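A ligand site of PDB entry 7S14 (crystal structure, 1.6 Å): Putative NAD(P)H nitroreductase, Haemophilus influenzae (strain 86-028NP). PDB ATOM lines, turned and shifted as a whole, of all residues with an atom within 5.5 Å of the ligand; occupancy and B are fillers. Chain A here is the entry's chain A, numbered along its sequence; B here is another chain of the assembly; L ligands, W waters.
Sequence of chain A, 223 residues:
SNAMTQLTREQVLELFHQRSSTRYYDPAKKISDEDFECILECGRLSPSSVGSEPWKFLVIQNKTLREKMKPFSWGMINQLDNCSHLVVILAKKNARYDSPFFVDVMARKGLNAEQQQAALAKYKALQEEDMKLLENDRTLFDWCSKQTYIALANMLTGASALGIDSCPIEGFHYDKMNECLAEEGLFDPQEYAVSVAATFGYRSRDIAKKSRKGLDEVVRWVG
Water W4 lies within hydrogen-bond range of O8 of the ligand (2.6 Å), OG of Ser 20 (2.7 Å) and N of Lys 210 (3.0 Å). Water W5 lies within hydrogen-bond range of O7 of the ligand (2.6 Å), O of Ser 21 (2.7 Å), NZ of Lys 210 (2.8 Å) and NH1 of Arg 23 (2.9 Å). Water W2 bridges an oxygen (O1) of the ligand (2.6 Å) and the backbone carbonyl oxygen (O) of Gly 75 (3.3 Å). Water W3 bridges O5 of the ligand (2.6 Å) and NH2 of Arg 23 (2.8 Å). Water W6 bridges an oxygen (O3) of the ligand and the backbone NH (N) of Val 50 of chain B.
The backbone carbonyl oxygen (O) of Pro 168 lies close to a nitrogen (N4) of the ligand (3.2 Å). Merely in contact with the ligand: Pro 47 of chain B, Ser 49 of chain B, Ser 48 of chain B, Ile 169, Lys 210, Ser 20, Ile 150 of chain B, Gln 147 of chain B, Tyr 149, Gly 51 of chain B, Val 50 of chain B and Gln 79. Hydrophobic or aromatic side chains within 4 Å of the ligand: Tyr 149, Pro 168, Ile 169, Pro 47 of chain B and Ile 150 of chain B. 21 residues have an atom within 4 Å of the ligand: Arg 19, Ser 20, Ser 21, Arg 23, Gly 75, Gln 79, Tyr 149, Cys 167, Pro 168, Ile 169, Glu 170, Gly 171, Lys 210, Arg 212, Pro 47 of chain B, Ser 48 of chain B, Ser 49 of chain B, Val 50 of chain B, Gly 51 of chain B, Gln 147 of chain B and Ile 150 of chain B. The nearest printed residue that does not touch the ligand is Val 196 (4.2 Å).
The guanidinium group (NH1) of Arg 23 lies within hydrogen-bond range of the backbone carbonyl oxygen (O) of Ser 21 (3.4 Å). The backbone carbonyl oxygen (O) of Leu 45 of chain B lies within hydrogen-bond range of the guanidinium group (NH2) of Arg 212, 3.1 Å away. The backbone NH of Gly 75 lies within hydrogen-bond range of the backbone carbonyl oxygen of Gly 171. The backbone NH (N) of Trp 74 is in hydrogen-bond range of the backbone carbonyl oxygen (O) of Gly 171 (3.2 Å). The side-chain carboxylate (OE1) of Glu 170 lies within hydrogen-bond range of the side-chain hydroxyl (OG) of Ser 49 of chain B, 2.7 Å away. The side-chain carboxylate (OE2) of Glu 170 lies within hydrogen-bond range of the side-chain hydroxyl (OH) of Tyr 149 (2.7 Å). The backbone NH (N) of Ser 49 of chain B sits at hydrogen-bond distance from the side-chain amide oxygen (OE1) of Gln 147 of chain B. NZ of Lys 210 lies within hydrogen-bond range of O of Ala 208 (2.7 Å).
O1 of the ligand is in hydrogen-bond range of NE of Arg 23, 2.7 Å away. An oxygen (O7) of the ligand is in hydrogen-bond range of the backbone NH (N) of Ser 21 (2.7 Å). The side-chain hydroxyl (OG) of Ser 21 sits at hydrogen-bond distance from an oxygen (O9) of the ligand (2.7 Å). NH2 of Arg 212 lies within salt-bridge range of O8 of the ligand (2.7 Å). O2 of the ligand lies within hydrogen-bond range of N of Gly 171, 2.8 Å away. O of Gly 75 is in hydrogen-bond range of N2 of the ligand, 2.9 Å away. O9 of the ligand is in salt-bridge range of NH2 of Arg 19 (2.9 Å). N of Glu 170 sits at hydrogen-bond distance from N3 of the ligand, 2.9 Å away. N1 of the ligand sits at hydrogen-bond distance from SG of Cys 167 (3.6 Å).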
ATOM      1  N   ARG A  19     -34.793 -21.135  12.067  1.00  0.00           N
ATOM      2  CA  ARG A  19     -33.755 -20.647  11.120  1.00  0.00           C
ATOM      3  C   ARG A  19     -32.845 -21.812  10.744  1.00  0.00           C
ATOM      4  O   ARG A  19     -32.175 -22.365  11.634  1.00  0.00           O
ATOM      5  CB  ARG A  19     -32.912 -19.508  11.700  1.00  0.00           C
ATOM      6  CG  ARG A  19     -31.909 -18.940  10.702  1.00  0.00           C
ATOM      7  CD  ARG A  19     -30.516 -18.712  11.278  1.00  0.00           C
ATOM      8  NE  ARG A  19     -29.987 -19.945  11.834  1.00  0.00           N
ATOM      9  CZ  ARG A  19     -29.215 -20.822  11.203  1.00  0.00           C
ATOM     10  NH1 ARG A  19     -28.830 -20.616   9.950  1.00  0.00           N
ATOM     11  NH2 ARG A  19     -28.803 -21.911  11.841  1.00  0.00           N
ATOM     12  N   SER A  20     -32.796 -22.151   9.455  1.00  0.00           N
ATOM     13  CA  SER A  20     -31.861 -23.158   8.893  1.00  0.00           C
ATOM     14  C   SER A  20     -31.049 -22.506   7.783  1.00  0.00           C
ATOM     15  O   SER A  20     -31.466 -21.462   7.228  1.00  0.00           O
ATOM     16  CB  SER A  20     -32.597 -24.390   8.416  1.00  0.00           C
ATOM     17  OG  SER A  20     -32.827 -25.297   9.490  1.00  0.00           O
ATOM     18  N   SER A  21     -29.889 -23.075   7.492  1.00  0.00           N
ATOM     19  CA  SER A  21     -29.047 -22.707   6.317  1.00  0.00           C
ATOM     20  C   SER A  21     -29.719 -23.256   5.050  1.00  0.00           C
ATOM     21  O   SER A  21     -29.872 -24.492   4.939  1.00  0.00           O
ATOM     22  CB  SER A  21     -27.638 -23.187   6.487  1.00  0.00           C
ATOM     23  OG  SER A  21     -27.006 -22.479   7.537  1.00  0.00           O
ATOM     24  N   ARG A  23     -29.935 -23.993   1.089  1.00  0.00           N
ATOM     25  CA  ARG A  23     -29.069 -24.236  -0.090  1.00  0.00           C
ATOM     26  C   ARG A  23     -29.904 -24.314  -1.370  1.00  0.00           C
ATOM     27  O   ARG A  23     -29.298 -24.301  -2.460  1.00  0.00           O
ATOM     28  CB  ARG A  23     -28.260 -25.510   0.126  1.00  0.00           C
ATOM     29  CG  ARG A  23     -27.229 -25.360   1.234  1.00  0.00           C
ATOM     30  CD  ARG A  23     -26.713 -26.690   1.748  1.00  0.00           C
ATOM     31  NE  ARG A  23     -25.816 -26.470   2.870  1.00  0.00           N
ATOM     32  CZ  ARG A  23     -26.138 -26.536   4.159  1.00  0.00           C
ATOM     33  NH1 ARG A  23     -27.371 -26.831   4.536  1.00  0.00           N
ATOM     34  NH2 ARG A  23     -25.217 -26.298   5.077  1.00  0.00           N
ATOM     35  N   TRP A  74     -17.607 -23.447  -4.607  1.00  0.00           N
ATOM     36  CA  TRP A  74     -18.256 -24.786  -4.497  1.00  0.00           C
ATOM     37  C   TRP A  74     -19.313 -24.784  -3.391  1.00  0.00           C
ATOM     38  O   TRP A  74     -20.298 -25.543  -3.527  1.00  0.00           O
ATOM     39  CB  TRP A  74     -17.206 -25.894  -4.280  1.00  0.00           C
ATOM     40  CG  TRP A  74     -16.247 -25.642  -3.166  1.00  0.00           C
ATOM     41  CD1 TRP A  74     -15.022 -25.047  -3.258  1.00  0.00           C
ATOM     42  CD2 TRP A  74     -16.408 -25.990  -1.777  1.00  0.00           C
ATOM     43  NE1 TRP A  74     -14.412 -24.993  -2.034  1.00  0.00           N
ATOM     44  CE2 TRP A  74     -15.240 -25.562  -1.109  1.00  0.00           C
ATOM     45  CE3 TRP A  74     -17.423 -26.611  -1.039  1.00  0.00           C
ATOM     46  CZ2 TRP A  74     -15.062 -25.746   0.263  1.00  0.00           C
ATOM     47  CZ3 TRP A  74     -17.242 -26.795   0.311  1.00  0.00           C
ATOM     48  CH2 TRP A  74     -16.072 -26.376   0.956  1.00  0.00           C
ATOM     49  N   GLY A  75     -19.139 -23.967  -2.346  1.00  0.00           N
ATOM     50  CA  GLY A  75     -20.065 -23.845  -1.204  1.00  0.00           C
ATOM     51  C   GLY A  75     -21.394 -23.223  -1.591  1.00  0.00           C
ATOM     52  O   GLY A  75     -22.347 -23.380  -0.820  1.00  0.00           O
ATOM     53  N   MET A  76     -21.481 -22.529  -2.729  1.00  0.00           N
ATOM     54  CA  MET A  76     -22.735 -21.845  -3.154  1.00  0.00           C
ATOM     55  C   MET A  76     -22.963 -22.010  -4.654  1.00  0.00           C
ATOM     56  O   MET A  76     -23.604 -21.123  -5.248  1.00  0.00           O
ATOM     57  CB  MET A  76     -22.691 -20.377  -2.739  1.00  0.00           C
ATOM     58  CG  MET A  76     -21.450 -19.642  -3.204  1.00  0.00           C
ATOM     59  SD  MET A  76     -21.602 -17.726  -2.848  1.00  0.00           S
ATOM     60  CE  MET A  76     -19.750 -17.089  -2.994  1.00  0.00           C
ATOM     61  N   GLN A  79     -26.606 -22.001  -5.374  1.00  0.00           N
ATOM     62  CA  GLN A  79     -27.243 -20.798  -4.762  1.00  0.00           C
ATOM     63  C   GLN A  79     -27.009 -19.578  -5.653  1.00  0.00           C
ATOM     64  O   GLN A  79     -27.933 -18.747  -5.770  1.00  0.00           O
ATOM     65  CB  GLN A  79     -26.700 -20.593  -3.349  1.00  0.00           C
ATOM     66  CG  GLN A  79     -27.039 -21.740  -2.412  1.00  0.00           C
ATOM     67  CD  GLN A  79     -26.428 -21.553  -1.049  1.00  0.00           C
ATOM     68  OE1 GLN A  79     -26.504 -20.471  -0.457  1.00  0.00           O
ATOM     69  NE2 GLN A  79     -25.788 -22.596  -0.547  1.00  0.00           N
ATOM     70  N   TYR A 149     -18.229 -11.372  11.574  1.00  0.00           N
ATOM     71  CA  TYR A 149     -19.073 -12.578  11.824  1.00  0.00           C
ATOM     72  C   TYR A 149     -20.234 -12.176  12.742  1.00  0.00           C
ATOM     73  O   TYR A 149     -21.278 -12.850  12.695  1.00  0.00           O
ATOM     74  CB  TYR A 149     -18.253 -13.742  12.371  1.00  0.00           C
ATOM     75  CG  TYR A 149     -17.552 -14.544  11.298  1.00  0.00           C
ATOM     76  CD1 TYR A 149     -16.594 -13.960  10.474  1.00  0.00           C
ATOM     77  CD2 TYR A 149     -17.854 -15.874  11.076  1.00  0.00           C
ATOM     78  CE1 TYR A 149     -15.947 -14.677   9.482  1.00  0.00           C
ATOM     79  CE2 TYR A 149     -17.223 -16.609  10.085  1.00  0.00           C
ATOM     80  CZ  TYR A 149     -16.268 -16.016   9.284  1.00  0.00           C
ATOM     81  OH  TYR A 149     -15.630 -16.723   8.309  1.00  0.00           O
ATOM     82  N   LEU A 152     -22.556 -10.697  10.156  1.00  0.00           N
ATOM     83  CA  LEU A 152     -23.123 -11.880   9.452  1.00  0.00           C
ATOM     84  C   LEU A 152     -24.307 -12.440  10.253  1.00  0.00           C
ATOM     85  O   LEU A 152     -25.417 -12.539   9.696  1.00  0.00           O
ATOM     86  CB  LEU A 152     -22.031 -12.931   9.270  1.00  0.00           C
ATOM     87  CG  LEU A 152     -22.490 -14.291   8.734  1.00  0.00           C
ATOM     88  CD1 LEU A 152     -22.926 -14.196   7.284  1.00  0.00           C
ATOM     89  CD2 LEU A 152     -21.390 -15.333   8.897  1.00  0.00           C
ATOM     90  N   CYS A 167     -28.234 -18.307   3.894  1.00  0.00           N
ATOM     91  CA  CYS A 167     -27.124 -19.271   4.098  1.00  0.00           C
ATOM     92  C   CYS A 167     -25.819 -18.490   4.259  1.00  0.00           C
ATOM     93  O   CYS A 167     -25.477 -17.711   3.378  1.00  0.00           O
ATOM     94  CB  CYS A 167     -27.008 -20.245   2.932  1.00  0.00           C
ATOM     95  SG  CYS A 167     -25.985 -21.691   3.291  1.00  0.00           S
ATOM     96  N   PRO A 168     -25.097 -18.659   5.387  1.00  0.00           N
ATOM     97  CA  PRO A 168     -23.729 -18.138   5.495  1.00  0.00           C
ATOM     98  C   PRO A 168     -22.826 -19.011   4.626  1.00  0.00           C
ATOM     99  O   PRO A 168     -23.125 -20.193   4.473  1.00  0.00           O
ATOM    100  CB  PRO A 168     -23.416 -18.248   6.994  1.00  0.00           C
ATOM    101  CG  PRO A 168     -24.279 -19.403   7.459  1.00  0.00           C
ATOM    102  CD  PRO A 168     -25.528 -19.334   6.616  1.00  0.00           C
ATOM    103  N   ILE A 169     -21.762 -18.437   4.070  1.00  0.00           N
ATOM    104  CA  ILE A 169     -20.928 -19.088   3.022  1.00  0.00           C
ATOM    105  C   ILE A 169     -19.448 -18.835   3.305  1.00  0.00           C
ATOM    106  O   ILE A 169     -19.027 -17.654   3.336  1.00  0.00           O
ATOM    107  CB  ILE A 169     -21.306 -18.578   1.618  1.00  0.00           C
ATOM    108  CG1 ILE A 169     -22.775 -18.859   1.260  1.00  0.00           C
ATOM    109  CG2 ILE A 169     -20.358 -19.145   0.572  1.00  0.00           C
ATOM    110  CD1 ILE A 169     -23.119 -20.329   1.112  1.00  0.00           C
ATOM    111  N   GLU A 170     -18.684 -19.928   3.457  1.00  0.00           N
ATOM    112  CA  GLU A 170     -17.203 -19.925   3.495  1.00  0.00           C
ATOM    113  C   GLU A 170     -16.640 -20.794   2.354  1.00  0.00           C
ATOM    114  O   GLU A 170     -15.401 -20.773   2.177  1.00  0.00           O
ATOM    115  CB  GLU A 170     -16.712 -20.477   4.834  1.00  0.00           C
ATOM    116  CG  GLU A 170     -16.501 -19.425   5.906  1.00  0.00           C
ATOM    117  CD  GLU A 170     -16.015 -20.055   7.195  1.00  0.00           C
ATOM    118  OE1 GLU A 170     -15.700 -21.264   7.164  1.00  0.00           O
ATOM    119  OE2 GLU A 170     -15.963 -19.362   8.222  1.00  0.00           O
ATOM    120  N   GLY A 171     -17.489 -21.530   1.642  1.00  0.00           N
ATOM    121  CA  GLY A 171     -17.071 -22.547   0.651  1.00  0.00           C
ATOM    122  C   GLY A 171     -16.689 -21.931  -0.682  1.00  0.00           C
ATOM    123  O   GLY A 171     -17.370 -22.209  -1.689  1.00  0.00           O
ATOM    124  N   PHE A 172     -15.635 -21.114  -0.683  1.00  0.00           N
ATOM    125  CA  PHE A 172     -15.021 -20.567  -1.926  1.00  0.00           C
ATOM    126  C   PHE A 172     -13.520 -20.385  -1.711  1.00  0.00           C
ATOM    127  O   PHE A 172     -13.068 -20.366  -0.535  1.00  0.00           O
ATOM    128  CB  PHE A 172     -15.685 -19.242  -2.336  1.00  0.00           C
ATOM    129  CG  PHE A 172     -15.706 -18.186  -1.266  1.00  0.00           C
ATOM    130  CD1 PHE A 172     -14.640 -17.330  -1.079  1.00  0.00           C
ATOM    131  CD2 PHE A 172     -16.818 -18.049  -0.436  1.00  0.00           C
ATOM    132  CE1 PHE A 172     -14.667 -16.360  -0.095  1.00  0.00           C
ATOM    133  CE2 PHE A 172     -16.844 -17.078   0.549  1.00  0.00           C
ATOM    134  CZ  PHE A 172     -15.775 -16.233   0.727  1.00  0.00           C
ATOM    135  N   VAL A 196     -16.315 -13.216   4.647  1.00  0.00           N
ATOM    136  CA  VAL A 196     -17.375 -14.264   4.630  1.00  0.00           C
ATOM    137  C   VAL A 196     -18.482 -13.776   3.696  1.00  0.00           C
ATOM    138  O   VAL A 196     -18.542 -12.559   3.453  1.00  0.00           O
ATOM    139  CB  VAL A 196     -17.865 -14.577   6.057  1.00  0.00           C
ATOM    140  CG1 VAL A 196     -18.577 -13.406   6.716  1.00  0.00           C
ATOM    141  CG2 VAL A 196     -18.729 -15.829   6.112  1.00  0.00           C
ATOM    142  N   ALA A 208     -34.638 -29.504   6.054  1.00  0.00           N
ATOM    143  CA  ALA A 208     -34.628 -30.285   7.314  1.00  0.00           C
ATOM    144  C   ALA A 208     -33.840 -29.509   8.371  1.00  0.00           C
ATOM    145  O   ALA A 208     -32.788 -28.935   8.026  1.00  0.00           O
ATOM    146  CB  ALA A 208     -34.030 -31.656   7.083  1.00  0.00           C
ATOM    147  N   LYS A 210     -31.273 -29.093  11.358  1.00  0.00           N
ATOM    148  CA  LYS A 210     -29.945 -29.732  11.514  1.00  0.00           C
ATOM    149  C   LYS A 210     -29.605 -29.886  12.998  1.00  0.00           C
ATOM    150  O   LYS A 210     -30.147 -29.135  13.830  1.00  0.00           O
ATOM    151  CB  LYS A 210     -28.871 -28.937  10.773  1.00  0.00           C
ATOM    152  CG  LYS A 210     -29.125 -28.775   9.276  1.00  0.00           C
ATOM    153  CD  LYS A 210     -29.407 -30.090   8.569  1.00  0.00           C
ATOM    154  CE  LYS A 210     -29.413 -29.954   7.062  1.00  0.00           C
ATOM    155  NZ  LYS A 210     -30.477 -29.032   6.588  1.00  0.00           N
ATOM    156  N   SER A 211     -28.730 -30.841  13.293  1.00  0.00           N
ATOM    157  CA  SER A 211     -28.371 -31.274  14.657  1.00  0.00           C
ATOM    158  C   SER A 211     -27.511 -30.204  15.337  1.00  0.00           C
ATOM    159  O   SER A 211     -26.803 -29.438  14.636  1.00  0.00           O
ATOM    160  CB  SER A 211     -27.684 -32.610  14.644  1.00  0.00           C
ATOM    161  OG  SER A 211     -26.412 -32.528  14.012  1.00  0.00           O
ATOM    162  N   ARG A 212     -27.594 -30.166  16.665  1.00  0.00           N
ATOM    163  CA  ARG A 212     -26.668 -29.420  17.552  1.00  0.00           C
ATOM    164  C   ARG A 212     -26.292 -30.332  18.729  1.00  0.00           C
ATOM    165  O   ARG A 212     -27.074 -31.258  19.070  1.00  0.00           O
ATOM    166  CB  ARG A 212     -27.308 -28.131  18.085  1.00  0.00           C
ATOM    167  CG  ARG A 212     -27.563 -27.072  17.021  1.00  0.00           C
ATOM    168  CD  ARG A 212     -26.308 -26.503  16.403  1.00  0.00           C
ATOM    169  NE  ARG A 212     -26.638 -25.374  15.552  1.00  0.00           N
ATOM    170  CZ  ARG A 212     -27.211 -25.455  14.356  1.00  0.00           C
ATOM    171  NH1 ARG A 212     -27.487 -26.640  13.817  1.00  0.00           N
ATOM    172  NH2 ARG A 212     -27.509 -24.352  13.699  1.00  0.00           N
ATOM    173  N   LEU B  45     -27.799 -22.751  19.266  1.00  0.00           N
ATOM    174  CA  LEU B  45     -28.574 -22.971  18.022  1.00  0.00           C
ATOM    175  C   LEU B  45     -27.943 -22.199  16.867  1.00  0.00           C
ATOM    176  O   LEU B  45     -28.484 -22.270  15.753  1.00  0.00           O
ATOM    177  CB  LEU B  45     -30.018 -22.529  18.244  1.00  0.00           C
ATOM    178  CG  LEU B  45     -30.818 -23.417  19.203  1.00  0.00           C
ATOM    179  CD1 LEU B  45     -32.238 -22.892  19.341  1.00  0.00           C
ATOM    180  CD2 LEU B  45     -30.827 -24.857  18.727  1.00  0.00           C
ATOM    181  N   PRO B  47     -25.607 -21.029  13.720  1.00  0.00           N
ATOM    182  CA  PRO B  47     -24.917 -21.716  12.623  1.00  0.00           C
ATOM    183  C   PRO B  47     -23.405 -21.648  12.862  1.00  0.00           C
ATOM    184  O   PRO B  47     -22.915 -20.791  13.625  1.00  0.00           O
ATOM    185  CB  PRO B  47     -25.334 -20.917  11.385  1.00  0.00           C
ATOM    186  CG  PRO B  47     -25.529 -19.522  11.929  1.00  0.00           C
ATOM    187  CD  PRO B  47     -26.145 -19.721  13.302  1.00  0.00           C
ATOM    188  N   SER B  48     -22.693 -22.556  12.204  1.00  0.00           N
ATOM    189  CA  SER B  48     -21.213 -22.664  12.247  1.00  0.00           C
ATOM    190  C   SER B  48     -20.743 -23.308  10.946  1.00  0.00           C
ATOM    191  O   SER B  48     -21.478 -24.150  10.379  1.00  0.00           O
ATOM    192  CB  SER B  48     -20.769 -23.416  13.477  1.00  0.00           C
ATOM    193  OG  SER B  48     -21.278 -24.738  13.464  1.00  0.00           O
ATOM    194  N   SER B  49     -19.573 -22.905  10.460  1.00  0.00           N
ATOM    195  CA  SER B  49     -18.940 -23.508   9.271  1.00  0.00           C
ATOM    196  C   SER B  49     -18.920 -25.029   9.438  1.00  0.00           C
ATOM    197  O   SER B  49     -18.503 -25.505  10.514  1.00  0.00           O
ATOM    198  CB  SER B  49     -17.566 -22.947   9.028  1.00  0.00           C
ATOM    199  OG  SER B  49     -17.032 -23.485   7.839  1.00  0.00           O
ATOM    200  N   VAL B  50     -19.450 -25.745   8.434  1.00  0.00           N
ATOM    201  CA  VAL B  50     -19.497 -27.231   8.335  1.00  0.00           C
ATOM    202  C   VAL B  50     -20.107 -27.840   9.608  1.00  0.00           C
ATOM    203  O   VAL B  50     -19.757 -29.003   9.927  1.00  0.00           O
ATOM    204  CB  VAL B  50     -18.108 -27.810   7.996  1.00  0.00           C
ATOM    205  CG1 VAL B  50     -17.582 -27.237   6.692  1.00  0.00           C
ATOM    206  CG2 VAL B  50     -17.080 -27.619   9.100  1.00  0.00           C
ATOM    207  N   GLY B  51     -21.007 -27.119  10.291  1.00  0.00           N
ATOM    208  CA  GLY B  51     -21.687 -27.584  11.509  1.00  0.00           C
ATOM    209  C   GLY B  51     -20.714 -27.921  12.623  1.00  0.00           C
ATOM    210  O   GLY B  51     -21.014 -28.795  13.453  1.00  0.00           O
ATOM    211  N   LYS B 109     -24.109 -35.647  12.169  1.00  0.00           N
ATOM    212  CA  LYS B 109     -24.770 -35.426  10.862  1.00  0.00           C
ATOM    213  C   LYS B 109     -25.354 -36.737  10.323  1.00  0.00           C
ATOM    214  O   LYS B 109     -26.128 -36.679   9.346  1.00  0.00           O
ATOM    215  CB  LYS B 109     -23.803 -34.833   9.849  1.00  0.00           C
ATOM    216  CG  LYS B 109     -23.391 -33.389  10.105  1.00  0.00           C
ATOM    217  CD  LYS B 109     -22.501 -32.831   9.017  1.00  0.00           C
ATOM    218  CE  LYS B 109     -21.798 -31.548   9.396  1.00  0.00           C
ATOM    219  NZ  LYS B 109     -20.618 -31.299   8.535  1.00  0.00           N
ATOM    220  N   GLN B 147     -16.358 -18.451  14.284  1.00  0.00           N
ATOM    221  CA  GLN B 147     -17.657 -19.152  14.488  1.00  0.00           C
ATOM    222  C   GLN B 147     -18.269 -18.692  15.820  1.00  0.00           C
ATOM    223  O   GLN B 147     -19.489 -18.445  15.865  1.00  0.00           O
ATOM    224  CB  GLN B 147     -17.502 -20.671  14.445  1.00  0.00           C
ATOM    225  CG  GLN B 147     -16.603 -21.196  13.338  1.00  0.00           C
ATOM    226  CD  GLN B 147     -16.898 -20.610  11.976  1.00  0.00           C
ATOM    227  OE1 GLN B 147     -18.051 -20.588  11.530  1.00  0.00           O
ATOM    228  NE2 GLN B 147     -15.869 -20.155  11.280  1.00  0.00           N
ATOM    229  N   ILE B 150     -20.468 -15.545  16.006  1.00  0.00           N
ATOM    230  CA  ILE B 150     -21.897 -15.769  15.624  1.00  0.00           C
ATOM    231  C   ILE B 150     -22.676 -16.121  16.889  1.00  0.00           C
ATOM    232  O   ILE B 150     -23.741 -15.503  17.147  1.00  0.00           O
ATOM    233  CB  ILE B 150     -22.029 -16.874  14.548  1.00  0.00           C
ATOM    234  CG1 ILE B 150     -21.152 -16.599  13.317  1.00  0.00           C
ATOM    235  CG2 ILE B 150     -23.478 -17.053  14.137  1.00  0.00           C
ATOM    236  CD1 ILE B 150     -21.077 -17.770  12.351  1.00  0.00           C
HETATM  237  N1  LIG L   1     -23.314 -23.994   3.978  1.00  0.00           N
HETATM  238  C1  LIG L   1     -23.066 -24.220   2.664  1.00  0.00           C
HETATM  239  O1  LIG L   1     -23.796 -24.946   1.996  1.00  0.00           O
HETATM  240  N2  LIG L   1     -21.973 -23.707   2.033  1.00  0.00           N
HETATM  241  C2  LIG L   1     -21.069 -22.905   2.684  1.00  0.00           C
HETATM  242  O2  LIG L   1     -20.075 -22.491   2.099  1.00  0.00           O
HETATM  243  C3  LIG L   1     -21.276 -22.679   4.063  1.00  0.00           C
HETATM  244  N3  LIG L   1     -20.401 -21.944   4.720  1.00  0.00           N
HETATM  245  C4  LIG L   1     -20.731 -21.551   5.983  1.00  0.00           C
HETATM  246  C5  LIG L   1     -19.903 -20.606   6.623  1.00  0.00           C
HETATM  247  C6  LIG L   1     -20.167 -20.163   7.893  1.00  0.00           C
HETATM  248  C7  LIG L   1     -19.203 -19.219   8.566  1.00  0.00           C
HETATM  249  C8  LIG L   1     -21.229 -20.746   8.620  1.00  0.00           C
HETATM  250  C9  LIG L   1     -21.559 -20.260  10.013  1.00  0.00           C
HETATM  251  C10 LIG L   1     -22.043 -21.686   8.015  1.00  0.00           C
HETATM  252  C11 LIG L   1     -21.843 -22.075   6.674  1.00  0.00           C
HETATM  253  N4  LIG L   1     -22.691 -22.955   5.993  1.00  0.00           N
HETATM  254  C12 LIG L   1     -22.470 -23.235   4.650  1.00  0.00           C
HETATM  255  C13 LIG L   1     -23.889 -23.494   6.661  1.00  0.00           C
HETATM  256  C14 LIG L   1     -23.545 -24.536   7.725  1.00  0.00           C
HETATM  257  O3  LIG L   1     -23.191 -25.778   7.101  1.00  0.00           O
HETATM  258  C15 LIG L   1     -24.722 -24.731   8.684  1.00  0.00           C
HETATM  259  O4  LIG L   1     -24.829 -23.579   9.531  1.00  0.00           O
HETATM  260  C16 LIG L   1     -24.626 -25.980   9.573  1.00  0.00           C
HETATM  261  O5  LIG L   1     -24.652 -27.156   8.768  1.00  0.00           O
HETATM  262  C17 LIG L   1     -25.754 -26.044  10.584  1.00  0.00           C
HETATM  263  O6  LIG L   1     -27.019 -26.162   9.873  1.00  0.00           O
HETATM  264  P1  LIG L   1     -28.149 -25.024  10.061  1.00  0.00           P
HETATM  265  O7  LIG L   1     -29.159 -25.239   8.959  1.00  0.00           O
HETATM  266  O8  LIG L   1     -28.753 -25.257  11.443  1.00  0.00           O
HETATM  267  O9  LIG L   1     -27.454 -23.673   9.958  1.00  0.00           O
HETATM  268  O   HOH W   1     -24.658 -29.768   9.686  1.00  0.00           O
HETATM  269  O   HOH W   2     -23.823 -26.231  -0.264  1.00  0.00           O
HETATM  270  O   HOH W   3     -26.542 -27.775   7.087  1.00  0.00           O
HETATM  271  O   HOH W   4     -31.161 -26.108  11.446  1.00  0.00           O
HETATM  272  O   HOH W   5     -29.334 -26.503   6.704  1.00  0.00           O
HETATM  273  O   HOH W   6     -20.702 -25.473   5.974  1.00  0.00           O
